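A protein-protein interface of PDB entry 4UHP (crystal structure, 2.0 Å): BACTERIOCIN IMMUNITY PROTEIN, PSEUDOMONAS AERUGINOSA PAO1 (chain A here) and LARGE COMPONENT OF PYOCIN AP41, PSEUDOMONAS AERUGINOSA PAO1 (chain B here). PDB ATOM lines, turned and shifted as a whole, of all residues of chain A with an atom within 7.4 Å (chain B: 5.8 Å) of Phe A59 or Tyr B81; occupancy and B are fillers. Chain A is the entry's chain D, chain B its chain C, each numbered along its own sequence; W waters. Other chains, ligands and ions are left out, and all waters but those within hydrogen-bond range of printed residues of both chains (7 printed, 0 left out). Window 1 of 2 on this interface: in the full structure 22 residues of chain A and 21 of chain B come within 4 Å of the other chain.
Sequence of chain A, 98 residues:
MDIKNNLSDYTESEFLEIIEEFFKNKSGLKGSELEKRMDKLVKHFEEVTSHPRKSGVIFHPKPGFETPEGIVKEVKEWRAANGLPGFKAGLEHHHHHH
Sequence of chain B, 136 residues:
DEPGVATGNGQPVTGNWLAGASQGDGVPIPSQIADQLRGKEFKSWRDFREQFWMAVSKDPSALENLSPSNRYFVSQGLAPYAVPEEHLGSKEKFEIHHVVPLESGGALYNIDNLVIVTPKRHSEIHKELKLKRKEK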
ATOM      1  N   PHE A  22      19.259   7.883 -15.826  1.00  0.00           N
ATOM      2  CA  PHE A  22      19.604   9.100 -15.097  1.00  0.00           C
ATOM      3  C   PHE A  22      18.612  10.230 -15.375  1.00  0.00           C
ATOM      4  O   PHE A  22      18.811  11.361 -14.933  1.00  0.00           O
ATOM      5  CB  PHE A  22      21.022   9.552 -15.454  1.00  0.00           C
ATOM      6  CG  PHE A  22      22.092   8.615 -14.977  1.00  0.00           C
ATOM      7  CD1 PHE A  22      22.624   8.738 -13.705  1.00  0.00           C
ATOM      8  CD2 PHE A  22      22.560   7.604 -15.798  1.00  0.00           C
ATOM      9  CE1 PHE A  22      23.605   7.874 -13.263  1.00  0.00           C
ATOM     10  CE2 PHE A  22      23.540   6.737 -15.361  1.00  0.00           C
ATOM     11  CZ  PHE A  22      24.063   6.871 -14.091  1.00  0.00           C
ATOM     12  N   PHE A  23      17.543   9.915 -16.099  1.00  0.00           N
ATOM     13  CA  PHE A  23      16.542  10.914 -16.462  1.00  0.00           C
ATOM     14  C   PHE A  23      15.126  10.424 -16.179  1.00  0.00           C
ATOM     15  O   PHE A  23      14.194  11.219 -16.095  1.00  0.00           O
ATOM     16  CB  PHE A  23      16.672  11.289 -17.941  1.00  0.00           C
ATOM     17  CG  PHE A  23      17.965  11.976 -18.280  1.00  0.00           C
ATOM     18  CD1 PHE A  23      19.104  11.241 -18.562  1.00  0.00           C
ATOM     19  CD2 PHE A  23      18.038  13.359 -18.326  1.00  0.00           C
ATOM     20  CE1 PHE A  23      20.297  11.872 -18.876  1.00  0.00           C
ATOM     21  CE2 PHE A  23      19.226  13.996 -18.641  1.00  0.00           C
ATOM     22  CZ  PHE A  23      20.358  13.250 -18.915  1.00  0.00           C
ATOM     23  N   GLU A  35      18.382   5.065  -4.784  1.00  0.00           N
ATOM     24  CA  GLU A  35      19.624   5.816  -4.668  1.00  0.00           C
ATOM     25  C   GLU A  35      20.843   4.907  -4.753  1.00  0.00           C
ATOM     26  O   GLU A  35      21.843   5.261  -5.375  1.00  0.00           O
ATOM     27  CB  GLU A  35      19.654   6.610  -3.362  1.00  0.00           C
ATOM     28  CG  GLU A  35      20.807   7.590  -3.284  1.00  0.00           C
ATOM     29  CD  GLU A  35      20.547   8.720  -2.314  1.00  0.00           C
ATOM     30  OE1 GLU A  35      19.636   8.584  -1.470  1.00  0.00           O
ATOM     31  OE2 GLU A  35      21.247   9.751  -2.403  1.00  0.00           O
ATOM     32  N   MET A  38      21.335   3.974  -8.359  1.00  0.00           N
ATOM     33  CA  MET A  38      21.919   5.078  -9.110  1.00  0.00           C
ATOM     34  C   MET A  38      23.375   5.291  -8.696  1.00  0.00           C
ATOM     35  O   MET A  38      24.218   5.627  -9.528  1.00  0.00           O
ATOM     36  CB  MET A  38      21.099   6.355  -8.920  1.00  0.00           C
ATOM     37  CG  MET A  38      19.648   6.227  -9.366  1.00  0.00           C
ATOM     38  SD  MET A  38      19.456   5.461 -10.996  1.00  0.00           S
ATOM     39  CE  MET A  38      20.339   6.627 -12.028  1.00  0.00           C
ATOM     40  N   ASP A  39      23.668   5.080  -7.413  1.00  0.00           N
ATOM     41  CA  ASP A  39      25.047   5.099  -6.930  1.00  0.00           C
ATOM     42  C   ASP A  39      25.894   4.106  -7.723  1.00  0.00           C
ATOM     43  O   ASP A  39      26.987   4.435  -8.185  1.00  0.00           O
ATOM     44  CB  ASP A  39      25.111   4.767  -5.435  1.00  0.00           C
ATOM     45  CG  ASP A  39      24.682   5.931  -4.554  1.00  0.00           C
ATOM     46  OD1 ASP A  39      24.111   6.906  -5.082  1.00  0.00           O
ATOM     47  OD2 ASP A  39      24.908   5.867  -3.326  1.00  0.00           O
ATOM     48  N   LYS A  40      25.371   2.894  -7.884  1.00  0.00           N
ATOM     49  CA  LYS A  40      26.067   1.842  -8.614  1.00  0.00           C
ATOM     50  C   LYS A  40      26.265   2.203 -10.085  1.00  0.00           C
ATOM     51  O   LYS A  40      27.318   1.929 -10.661  1.00  0.00           O
ATOM     52  CB  LYS A  40      25.303   0.521  -8.506  1.00  0.00           C
ATOM     53  CG  LYS A  40      25.968  -0.633  -9.243  1.00  0.00           C
ATOM     54  CD  LYS A  40      25.055  -1.844  -9.343  1.00  0.00           C
ATOM     55  CE  LYS A  40      25.699  -2.942 -10.174  1.00  0.00           C
ATOM     56  NZ  LYS A  40      24.799  -4.115 -10.342  1.00  0.00           N
ATOM     57  N   LEU A  41      25.248   2.812 -10.687  1.00  0.00           N
ATOM     58  CA  LEU A  41      25.301   3.161 -12.105  1.00  0.00           C
ATOM     59  C   LEU A  41      26.306   4.278 -12.371  1.00  0.00           C
ATOM     60  O   LEU A  41      27.028   4.248 -13.368  1.00  0.00           O
ATOM     61  CB  LEU A  41      23.916   3.568 -12.611  1.00  0.00           C
ATOM     62  CG  LEU A  41      22.848   2.471 -12.638  1.00  0.00           C
ATOM     63  CD1 LEU A  41      21.562   2.999 -13.250  1.00  0.00           C
ATOM     64  CD2 LEU A  41      23.347   1.250 -13.393  1.00  0.00           C
ATOM     65  N   VAL A  42      26.345   5.261 -11.477  1.00  0.00           N
ATOM     66  CA  VAL A  42      27.296   6.365 -11.581  1.00  0.00           C
ATOM     67  C   VAL A  42      28.736   5.872 -11.543  1.00  0.00           C
ATOM     68  O   VAL A  42      29.547   6.219 -12.400  1.00  0.00           O
ATOM     69  CB  VAL A  42      27.109   7.394 -10.447  1.00  0.00           C
ATOM     70  CG1 VAL A  42      28.318   8.320 -10.364  1.00  0.00           C
ATOM     71  CG2 VAL A  42      25.834   8.189 -10.648  1.00  0.00           C
ATOM     72  N   LYS A  43      29.054   5.064 -10.538  1.00  0.00           N
ATOM     73  CA  LYS A  43      30.423   4.608 -10.357  1.00  0.00           C
ATOM     74  C   LYS A  43      30.803   3.628 -11.457  1.00  0.00           C
ATOM     75  O   LYS A  43      31.966   3.542 -11.842  1.00  0.00           O
ATOM     76  CB  LYS A  43      30.606   3.987  -8.970  1.00  0.00           C
ATOM     77  CG  LYS A  43      30.309   4.963  -7.831  1.00  0.00           C
ATOM     78  CD  LYS A  43      30.838   6.360  -8.161  1.00  0.00           C
ATOM     79  CE  LYS A  43      30.959   7.245  -6.931  1.00  0.00           C
ATOM     80  NZ  LYS A  43      32.206   8.058  -6.969  1.00  0.00           N
ATOM     81  N   GLU A  46      31.629   5.898 -14.514  1.00  0.00           N
ATOM     82  CA  GLU A  46      32.978   6.438 -14.374  1.00  0.00           C
ATOM     83  C   GLU A  46      34.045   5.379 -14.629  1.00  0.00           C
ATOM     84  O   GLU A  46      35.108   5.665 -15.185  1.00  0.00           O
ATOM     85  CB  GLU A  46      33.161   7.041 -12.981  1.00  0.00           C
ATOM     86  CG  GLU A  46      32.141   8.111 -12.654  1.00  0.00           C
ATOM     87  CD  GLU A  46      32.253   8.627 -11.235  1.00  0.00           C
ATOM     88  OE1 GLU A  46      32.871   7.945 -10.387  1.00  0.00           O
ATOM     89  OE2 GLU A  46      31.714   9.720 -10.972  1.00  0.00           O
ATOM     90  N   ARG A  53      36.015  13.836 -16.430  1.00  0.00           N
ATOM     91  CA  ARG A  53      34.985  14.577 -15.707  1.00  0.00           C
ATOM     92  C   ARG A  53      34.059  13.647 -14.920  1.00  0.00           C
ATOM     93  O   ARG A  53      33.157  14.112 -14.228  1.00  0.00           O
ATOM     94  CB  ARG A  53      34.164  15.441 -16.673  1.00  0.00           C
ATOM     95  CG  ARG A  53      34.986  16.473 -17.437  1.00  0.00           C
ATOM     96  CD  ARG A  53      34.101  17.505 -18.128  1.00  0.00           C
ATOM     97  NE  ARG A  53      33.359  18.316 -17.165  1.00  0.00           N
ATOM     98  CZ  ARG A  53      32.034  18.318 -17.046  1.00  0.00           C
ATOM     99  NH1 ARG A  53      31.291  17.564 -17.846  1.00  0.00           N
ATOM    100  NH2 ARG A  53      31.448  19.084 -16.134  1.00  0.00           N
ATOM    101  N   LYS A  54      34.291  12.340 -15.036  1.00  0.00           N
ATOM    102  CA  LYS A  54      33.524  11.328 -14.303  1.00  0.00           C
ATOM    103  C   LYS A  54      32.011  11.514 -14.468  1.00  0.00           C
ATOM    104  O   LYS A  54      31.512  11.619 -15.588  1.00  0.00           O
ATOM    105  CB  LYS A  54      33.898  11.347 -12.817  1.00  0.00           C
ATOM    106  CG  LYS A  54      35.362  11.021 -12.535  1.00  0.00           C
ATOM    107  CD  LYS A  54      35.627  10.914 -11.037  1.00  0.00           C
ATOM    108  CE  LYS A  54      35.271  12.212 -10.319  1.00  0.00           C
ATOM    109  NZ  LYS A  54      35.412  12.111  -8.837  1.00  0.00           N
ATOM    110  N   SER A  55      31.291  11.570 -13.350  1.00  0.00           N
ATOM    111  CA  SER A  55      29.839  11.747 -13.377  1.00  0.00           C
ATOM    112  C   SER A  55      29.446  13.133 -13.887  1.00  0.00           C
ATOM    113  O   SER A  55      28.284  13.382 -14.206  1.00  0.00           O
ATOM    114  CB  SER A  55      29.242  11.523 -11.986  1.00  0.00           C
ATOM    115  OG  SER A  55      29.615  12.570 -11.111  1.00  0.00           O
ATOM    116  N   GLY A  56      30.425  14.032 -13.955  1.00  0.00           N
ATOM    117  CA  GLY A  56      30.209  15.366 -14.480  1.00  0.00           C
ATOM    118  C   GLY A  56      29.639  15.366 -15.885  1.00  0.00           C
ATOM    119  O   GLY A  56      28.907  16.280 -16.253  1.00  0.00           O
ATOM    120  N   VAL A  57      29.968  14.344 -16.671  1.00  0.00           N
ATOM    121  CA  VAL A  57      29.415  14.215 -18.016  1.00  0.00           C
ATOM    122  C   VAL A  57      27.891  14.137 -17.952  1.00  0.00           C
ATOM    123  O   VAL A  57      27.188  14.718 -18.779  1.00  0.00           O
ATOM    124  CB  VAL A  57      29.957  12.969 -18.741  1.00  0.00           C
ATOM    125  CG1 VAL A  57      29.363  12.866 -20.139  1.00  0.00           C
ATOM    126  CG2 VAL A  57      31.482  13.010 -18.806  1.00  0.00           C
ATOM    127  N   ILE A  58      27.390  13.427 -16.949  1.00  0.00           N
ATOM    128  CA  ILE A  58      25.954  13.249 -16.769  1.00  0.00           C
ATOM    129  C   ILE A  58      25.301  14.437 -16.074  1.00  0.00           C
ATOM    130  O   ILE A  58      24.331  15.008 -16.582  1.00  0.00           O
ATOM    131  CB  ILE A  58      25.650  11.980 -15.948  1.00  0.00           C
ATOM    132  CG1 ILE A  58      26.200  10.740 -16.652  1.00  0.00           C
ATOM    133  CG2 ILE A  58      24.155  11.849 -15.700  1.00  0.00           C
ATOM    134  CD1 ILE A  58      26.030   9.464 -15.851  1.00  0.00           C
ATOM    135  N   PHE A  59      25.836  14.805 -14.912  1.00  0.00           N
ATOM    136  CA  PHE A  59      25.175  15.768 -14.037  1.00  0.00           C
ATOM    137  C   PHE A  59      25.591  17.219 -14.282  1.00  0.00           C
ATOM    138  O   PHE A  59      24.904  18.142 -13.850  1.00  0.00           O
ATOM    139  CB  PHE A  59      25.432  15.403 -12.571  1.00  0.00           C
ATOM    140  CG  PHE A  59      24.914  14.044 -12.185  1.00  0.00           C
ATOM    141  CD1 PHE A  59      23.555  13.823 -12.040  1.00  0.00           C
ATOM    142  CD2 PHE A  59      25.786  12.994 -11.960  1.00  0.00           C
ATOM    143  CE1 PHE A  59      23.073  12.574 -11.681  1.00  0.00           C
ATOM    144  CE2 PHE A  59      25.312  11.745 -11.599  1.00  0.00           C
ATOM    145  CZ  PHE A  59      23.951  11.535 -11.460  1.00  0.00           C
ATOM    146  N   HIS A  60      26.719  17.424 -14.952  1.00  0.00           N
ATOM    147  CA  HIS A  60      27.138  18.774 -15.320  1.00  0.00           C
ATOM    148  C   HIS A  60      27.635  18.835 -16.763  1.00  0.00           C
ATOM    149  O   HIS A  60      28.786  19.194 -17.018  1.00  0.00           O
ATOM    150  CB  HIS A  60      28.207  19.270 -14.353  1.00  0.00           C
ATOM    151  CG  HIS A  60      27.715  19.395 -12.944  1.00  0.00           C
ATOM    152  ND1 HIS A  60      27.138  20.550 -12.459  1.00  0.00           N
ATOM    153  CD2 HIS A  60      27.679  18.502 -11.928  1.00  0.00           C
ATOM    154  CE1 HIS A  60      26.784  20.367 -11.199  1.00  0.00           C
ATOM    155  NE2 HIS A  60      27.100  19.132 -10.853  1.00  0.00           N
ATOM    156  N   PRO A  61      26.751  18.495 -17.712  1.00  0.00           N
ATOM    157  CA  PRO A  61      27.130  18.341 -19.117  1.00  0.00           C
ATOM    158  C   PRO A  61      27.415  19.668 -19.809  1.00  0.00           C
ATOM    159  O   PRO A  61      26.898  20.710 -19.402  1.00  0.00           O
ATOM    160  CB  PRO A  61      25.902  17.669 -19.728  1.00  0.00           C
ATOM    161  CG  PRO A  61      24.770  18.201 -18.914  1.00  0.00           C
ATOM    162  CD  PRO A  61      25.296  18.340 -17.516  1.00  0.00           C
ATOM    163  N   GLU A  66      23.288  17.678 -22.876  1.00  0.00           N
ATOM    164  CA  GLU A  66      22.568  17.445 -21.622  1.00  0.00           C
ATOM    165  C   GLU A  66      21.688  16.200 -21.648  1.00  0.00           C
ATOM    166  O   GLU A  66      21.318  15.670 -20.600  1.00  0.00           O
ATOM    167  CB  GLU A  66      21.696  18.655 -21.270  1.00  0.00           C
ATOM    168  CG  GLU A  66      22.461  19.949 -21.063  1.00  0.00           C
ATOM    169  CD  GLU A  66      22.585  20.769 -22.331  1.00  0.00           C
ATOM    170  OE1 GLU A  66      22.296  20.234 -23.424  1.00  0.00           O
ATOM    171  OE2 GLU A  66      22.961  21.956 -22.231  1.00  0.00           O
ATOM    172  N   ILE A  71      25.223  12.717 -23.793  1.00  0.00           N
ATOM    173  CA  ILE A  71      26.137  12.055 -22.867  1.00  0.00           C
ATOM    174  C   ILE A  71      26.893  10.922 -23.562  1.00  0.00           C
ATOM    175  O   ILE A  71      28.115  10.809 -23.443  1.00  0.00           O
ATOM    176  CB  ILE A  71      25.386  11.494 -21.648  1.00  0.00           C
ATOM    177  CG1 ILE A  71      24.738  12.636 -20.861  1.00  0.00           C
ATOM    178  CG2 ILE A  71      26.330  10.697 -20.763  1.00  0.00           C
ATOM    179  CD1 ILE A  71      23.864  12.183 -19.719  1.00  0.00           C
ATOM    180  N   SER B  67      21.134  20.703 -13.913  1.00  0.00           N
ATOM    181  CA  SER B  67      21.054  19.956 -15.161  1.00  0.00           C
ATOM    182  C   SER B  67      19.798  19.095 -15.176  1.00  0.00           C
ATOM    183  O   SER B  67      19.288  18.737 -14.114  1.00  0.00           O
ATOM    184  CB  SER B  67      22.289  19.074 -15.329  1.00  0.00           C
ATOM    185  OG  SER B  67      22.349  18.119 -14.283  1.00  0.00           O
ATOM    186  N   SER B  69      19.502  16.066 -15.607  1.00  0.00           N
ATOM    187  CA  SER B  69      19.766  14.858 -14.832  1.00  0.00           C
ATOM    188  C   SER B  69      19.589  15.110 -13.332  1.00  0.00           C
ATOM    189  O   SER B  69      18.925  14.337 -12.640  1.00  0.00           O
ATOM    190  CB  SER B  69      21.174  14.331 -15.118  1.00  0.00           C
ATOM    191  OG  SER B  69      21.377  13.081 -14.483  1.00  0.00           O
ATOM    192  N   ASN B  70      20.175  16.193 -12.829  1.00  0.00           N
ATOM    193  CA  ASN B  70      20.016  16.535 -11.418  1.00  0.00           C
ATOM    194  C   ASN B  70      18.574  16.894 -11.074  1.00  0.00           C
ATOM    195  O   ASN B  70      18.139  16.703  -9.940  1.00  0.00           O
ATOM    196  CB  ASN B  70      20.949  17.684 -11.023  1.00  0.00           C
ATOM    197  CG  ASN B  70      22.263  17.190 -10.438  1.00  0.00           C
ATOM    198  OD1 ASN B  70      22.343  16.074  -9.931  1.00  0.00           O
ATOM    199  ND2 ASN B  70      23.298  18.022 -10.504  1.00  0.00           N
ATOM    200  N   PHE B  73      16.821  13.630 -10.423  1.00  0.00           N
ATOM    201  CA  PHE B  73      17.253  13.059  -9.154  1.00  0.00           C
ATOM    202  C   PHE B  73      16.528  13.685  -7.970  1.00  0.00           C
ATOM    203  O   PHE B  73      15.972  12.970  -7.138  1.00  0.00           O
ATOM    204  CB  PHE B  73      18.766  13.208  -8.989  1.00  0.00           C
ATOM    205  CG  PHE B  73      19.541  12.032  -9.508  1.00  0.00           C
ATOM    206  CD1 PHE B  73      19.465  11.677 -10.841  1.00  0.00           C
ATOM    207  CD2 PHE B  73      20.341  11.279  -8.662  1.00  0.00           C
ATOM    208  CE1 PHE B  73      20.174  10.587 -11.326  1.00  0.00           C
ATOM    209  CE2 PHE B  73      21.048  10.195  -9.140  1.00  0.00           C
ATOM    210  CZ  PHE B  73      20.966   9.849 -10.473  1.00  0.00           C
ATOM    211  N   ALA B  79      19.720  13.031  -3.612  1.00  0.00           N
ATOM    212  CA  ALA B  79      20.656  14.149  -3.576  1.00  0.00           C
ATOM    213  C   ALA B  79      21.284  14.366  -4.944  1.00  0.00           C
ATOM    214  O   ALA B  79      21.672  13.406  -5.612  1.00  0.00           O
ATOM    215  CB  ALA B  79      21.733  13.910  -2.530  1.00  0.00           C
ATOM    216  N   PRO B  80      21.376  15.634  -5.373  1.00  0.00           N
ATOM    217  CA  PRO B  80      22.015  15.968  -6.649  1.00  0.00           C
ATOM    218  C   PRO B  80      23.534  15.874  -6.557  1.00  0.00           C
ATOM    219  O   PRO B  80      24.085  15.923  -5.461  1.00  0.00           O
ATOM    220  CB  PRO B  80      21.569  17.411  -6.894  1.00  0.00           C
ATOM    221  CG  PRO B  80      21.380  17.964  -5.532  1.00  0.00           C
ATOM    222  CD  PRO B  80      20.846  16.828  -4.696  1.00  0.00           C
ATOM    223  N   TYR B  81      24.194  15.748  -7.702  1.00  0.00           N
ATOM    224  CA  TYR B  81      25.645  15.622  -7.741  1.00  0.00           C
ATOM    225  C   TYR B  81      26.315  16.969  -7.988  1.00  0.00           C
ATOM    226  O   TYR B  81      25.857  17.758  -8.810  1.00  0.00           O
ATOM    227  CB  TYR B  81      26.059  14.622  -8.823  1.00  0.00           C
ATOM    228  CG  TYR B  81      25.845  13.179  -8.433  1.00  0.00           C
ATOM    229  CD1 TYR B  81      24.566  12.660  -8.284  1.00  0.00           C
ATOM    230  CD2 TYR B  81      26.925  12.332  -8.217  1.00  0.00           C
ATOM    231  CE1 TYR B  81      24.369  11.339  -7.930  1.00  0.00           C
ATOM    232  CE2 TYR B  81      26.738  11.012  -7.862  1.00  0.00           C
ATOM    233  CZ  TYR B  81      25.458  10.520  -7.720  1.00  0.00           C
ATOM    234  OH  TYR B  81      25.268   9.205  -7.367  1.00  0.00           O
ATOM    235  N   ALA B  82      27.410  17.224  -7.281  1.00  0.00           N
ATOM    236  CA  ALA B  82      28.169  18.452  -7.484  1.00  0.00           C
ATOM    237  C   ALA B  82      29.131  18.305  -8.658  1.00  0.00           C
ATOM    238  O   ALA B  82      29.338  17.198  -9.165  1.00  0.00           O
ATOM    239  CB  ALA B  82      28.925  18.822  -6.222  1.00  0.00           C
ATOM    240  N   VAL B  83      29.707  19.423  -9.092  1.00  0.00           N
ATOM    241  CA  VAL B  83      30.702  19.408 -10.161  1.00  0.00           C
ATOM    242  C   VAL B  83      31.900  18.568  -9.730  1.00  0.00           C
ATOM    243  O   VAL B  83      32.187  18.472  -8.537  1.00  0.00           O
ATOM    244  CB  VAL B  83      31.173  20.839 -10.538  1.00  0.00           C
ATOM    245  CG1 VAL B  83      30.020  21.650 -11.115  1.00  0.00           C
ATOM    246  CG2 VAL B  83      31.793  21.545  -9.341  1.00  0.00           C
ATOM    247  N   HIS B  87      34.268  17.318  -5.927  1.00  0.00           N
ATOM    248  CA  HIS B  87      34.199  15.951  -5.419  1.00  0.00           C
ATOM    249  C   HIS B  87      35.291  15.688  -4.383  1.00  0.00           C
ATOM    250  O   HIS B  87      36.266  16.433  -4.289  1.00  0.00           O
ATOM    251  CB  HIS B  87      34.313  14.943  -6.563  1.00  0.00           C
ATOM    252  CG  HIS B  87      33.117  14.911  -7.462  1.00  0.00           C
ATOM    253  ND1 HIS B  87      33.037  14.094  -8.568  1.00  0.00           N
ATOM    254  CD2 HIS B  87      31.951  15.598  -7.415  1.00  0.00           C
ATOM    255  CE1 HIS B  87      31.874  14.279  -9.166  1.00  0.00           C
ATOM    256  NE2 HIS B  87      31.196  15.187  -8.488  1.00  0.00           N
ATOM    257  N   GLU B  92      30.473  12.574  -3.996  1.00  0.00           N
ATOM    258  CA  GLU B  92      30.154  13.454  -5.117  1.00  0.00           C
ATOM    259  C   GLU B  92      28.863  14.249  -4.941  1.00  0.00           C
ATOM    260  O   GLU B  92      28.644  15.241  -5.637  1.00  0.00           O
ATOM    261  CB  GLU B  92      30.064  12.637  -6.409  1.00  0.00           C
ATOM    262  CG  GLU B  92      31.302  11.809  -6.710  1.00  0.00           C
ATOM    263  CD  GLU B  92      31.218  11.109  -8.048  1.00  0.00           C
ATOM    264  OE1 GLU B  92      30.199  11.284  -8.749  1.00  0.00           O
ATOM    265  OE2 GLU B  92      32.178  10.395  -8.402  1.00  0.00           O
ATOM    266  N   LYS B  93      28.012  13.813  -4.016  1.00  0.00           N
ATOM    267  CA  LYS B  93      26.693  14.413  -3.849  1.00  0.00           C
ATOM    268  C   LYS B  93      26.718  15.653  -2.968  1.00  0.00           C
ATOM    269  O   LYS B  93      27.538  15.761  -2.057  1.00  0.00           O
ATOM    270  CB  LYS B  93      25.718  13.404  -3.241  1.00  0.00           C
ATOM    271  CG  LYS B  93      25.649  12.067  -3.942  1.00  0.00           C
ATOM    272  CD  LYS B  93      24.789  11.104  -3.136  1.00  0.00           C
ATOM    273  CE  LYS B  93      24.876   9.692  -3.681  1.00  0.00           C
ATOM    274  NZ  LYS B  93      24.097   8.737  -2.848  1.00  0.00           N
ATOM    275  N   PHE B  94      25.807  16.582  -3.243  1.00  0.00           N
ATOM    276  CA  PHE B  94      25.535  17.671  -2.314  1.00  0.00           C
ATOM    277  C   PHE B  94      25.078  17.063  -0.994  1.00  0.00           C
ATOM    278  O   PHE B  94      24.349  16.072  -0.985  1.00  0.00           O
ATOM    279  CB  PHE B  94      24.470  18.624  -2.863  1.00  0.00           C
ATOM    280  CG  PHE B  94      24.957  19.513  -3.973  1.00  0.00           C
ATOM    281  CD1 PHE B  94      25.631  20.691  -3.690  1.00  0.00           C
ATOM    282  CD2 PHE B  94      24.723  19.182  -5.300  1.00  0.00           C
ATOM    283  CE1 PHE B  94      26.073  21.518  -4.707  1.00  0.00           C
ATOM    284  CE2 PHE B  94      25.162  20.003  -6.324  1.00  0.00           C
ATOM    285  CZ  PHE B  94      25.837  21.173  -6.028  1.00  0.00           C
HETATM  286  O   HOH W   1      29.045  15.315 -11.438  1.00  0.00           O
HETATM  287  O   HOH W   2      18.850  11.696  -0.850  1.00  0.00           O
HETATM  288  O   HOH W   3      23.488  20.157 -12.436  1.00  0.00           O
HETATM  289  O   HOH W   4      22.859   8.714  -6.625  1.00  0.00           O
HETATM  290  O   HOH W   5      21.576  10.542  -5.337  1.00  0.00           O
HETATM  291  O   HOH W   6      21.808  16.295 -17.889  1.00  0.00           O
HETATM  292  O   HOH W   7      23.001   6.190  -1.278  1.00  0.00           O
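The backbone carbonyl oxygen of Ala B82 sits close to a ring nitrogen (NE2) of His A60 (3.4 Å).
OE2 of Glu B92 sits close to OE2 of Glu A46, at 2.7 Å.
The side-chain hydroxyl of Ser B69 lies within hydrogen-bond range of the backbone carbonyl oxygen of Phe A22.
The side-chain carboxylate (OD1) of Asp A39 is in salt-bridge range of the side-chain amino group (NZ) of Lys B93 (2.9 Å).
The side-chain hydroxyl (OG) of Ser B67 sits at hydrogen-bond distance from the backbone carbonyl oxygen (O) of Phe A59 (2.6 Å).
The side-chain amino group (NZ) of Lys A54 sits at hydrogen-bond distance from a ring nitrogen (ND1) of His B87, 3.1 Å away.
N of Val B83 sits at hydrogen-bond distance from NE2 of His A60 (3.2 Å).
The side-chain carboxylate (OE2) of Glu B92 lies within salt-bridge range of the side-chain amino group (NZ) of Lys A54, at 3.7 Å.
The side-chain amino group of Lys B93 lies within salt-bridge range of the side-chain carboxylate of Glu A35, at 3.1 Å.
O of Tyr B81 is in hydrogen-bond range of NE2 of His A60, 2.8 Å away.
OH of Tyr B81 lies within hydrogen-bond range of OD1 of Asp A39, at 3.4 Å.
The side-chain carboxylate (OE2) of Glu B92 is in salt-bridge range of the side-chain amino group (NZ) of Lys A43, at 2.7 Å.
OE1 of Glu B92 lies within hydrogen-bond range of OG of Ser A55, 2.8 Å away.
The backbone NH of Ala B82 lies within hydrogen-bond range of the backbone carbonyl oxygen of Glu B92.
The backbone NH (N) of Ser A55 is in hydrogen-bond range of the side-chain carboxylate (OE2) of Glu A46 (3.0 Å).
The guanidinium group (NH2) of Arg A53 sits at hydrogen-bond distance from the backbone carbonyl oxygen (O) of His A60 (2.8 Å).
O of Val B83 lies close to NE2 of His B87, at 3.4 Å.
The backbone carbonyl oxygen (O) of Ala B82 is in hydrogen-bond range of a ring nitrogen (NE2) of His B87 (2.8 Å).
CD1 of Phe A22 touches CZ of Phe B73, at 3.8 Å.
CE2 of Phe A23 touches N of Ser B69, at 3.7 Å.
Ala B79 touches Glu A35 (N to OE2, 3.8 Å).
CG1 of Val A42 touches OE1 of Glu B92, at 3.9 Å.
Tyr B81 touches Ser A55.
His B87 touches Ser A55 (CE1 to OG, 3.4 Å).
Phe A59 touches Ser B69 (CE1 to OG, 3.3 Å).
Phe A59 touches Phe B73.
Asn B70 touches His A60.
CB of Ser B67 touches CD of Pro A61, 3.8 Å away.
Phe A59 touches just these residues of chain B: Ser B67 (2.6 Å), Ser B69 (3.3 Å), Asn B70 (3.3 Å), Phe B73 (3.5 Å) and Tyr B81 (3.4 Å).
Tyr B81 touches five residues of chain A.
Of the printed residues of chain B, Lys A43 touches Glu B92 (2.7 Å).
Printed residues of chain A within 4 Å of Ser B69: Phe A22, Phe A23, Ile A58 and Phe A59.
The nearest residue of chain A that does not touch Tyr B81 is Met A38 (4.3 Å).
Of the 13 printed residues of chain B, 11 touch a printed residue of chain A.
Of the 21 printed residues of chain A, 14 touch a printed residue of chain B.
Hydrophobic or aromatic side chains of chain A that line the printed part of chain B: Phe A22, Phe A23, Met A38, Val A42, Ile A58, Phe A59, His A60 and Pro A61.
Among the printed residues, Asp or Glu carboxylates within 4 Å of a Lys or Arg side-chain nitrogen of the other chain: Glu A35 with Lys B93 (3.1 Å), Asp A39 with Lys B93 (2.9 Å), Lys A43 with Glu B92 (2.7 Å) and Lys A54 with Glu B92 (3.7 Å).
Water W4 lies within hydrogen-bond range of OH of Tyr B81 (2.6 Å) and OD1 of Asp A39 (2.7 Å).
Water W7 bridges the side-chain carboxylate (OD2) of Asp A39 (2.8 Å) and the side-chain amino group (NZ) of Lys B93 (3.2 Å).
Water W6 lies within hydrogen-bond range of O of Glu A66 (2.8 Å), O of Ile A58 (3.1 Å) and N of Ser B69 (3.3 Å).
Water W5 bridges the backbone carbonyl oxygen (O) of Ala B79 (2.9 Å) and the side-chain carboxylate (OE2) of Glu A35 (3.1 Å).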
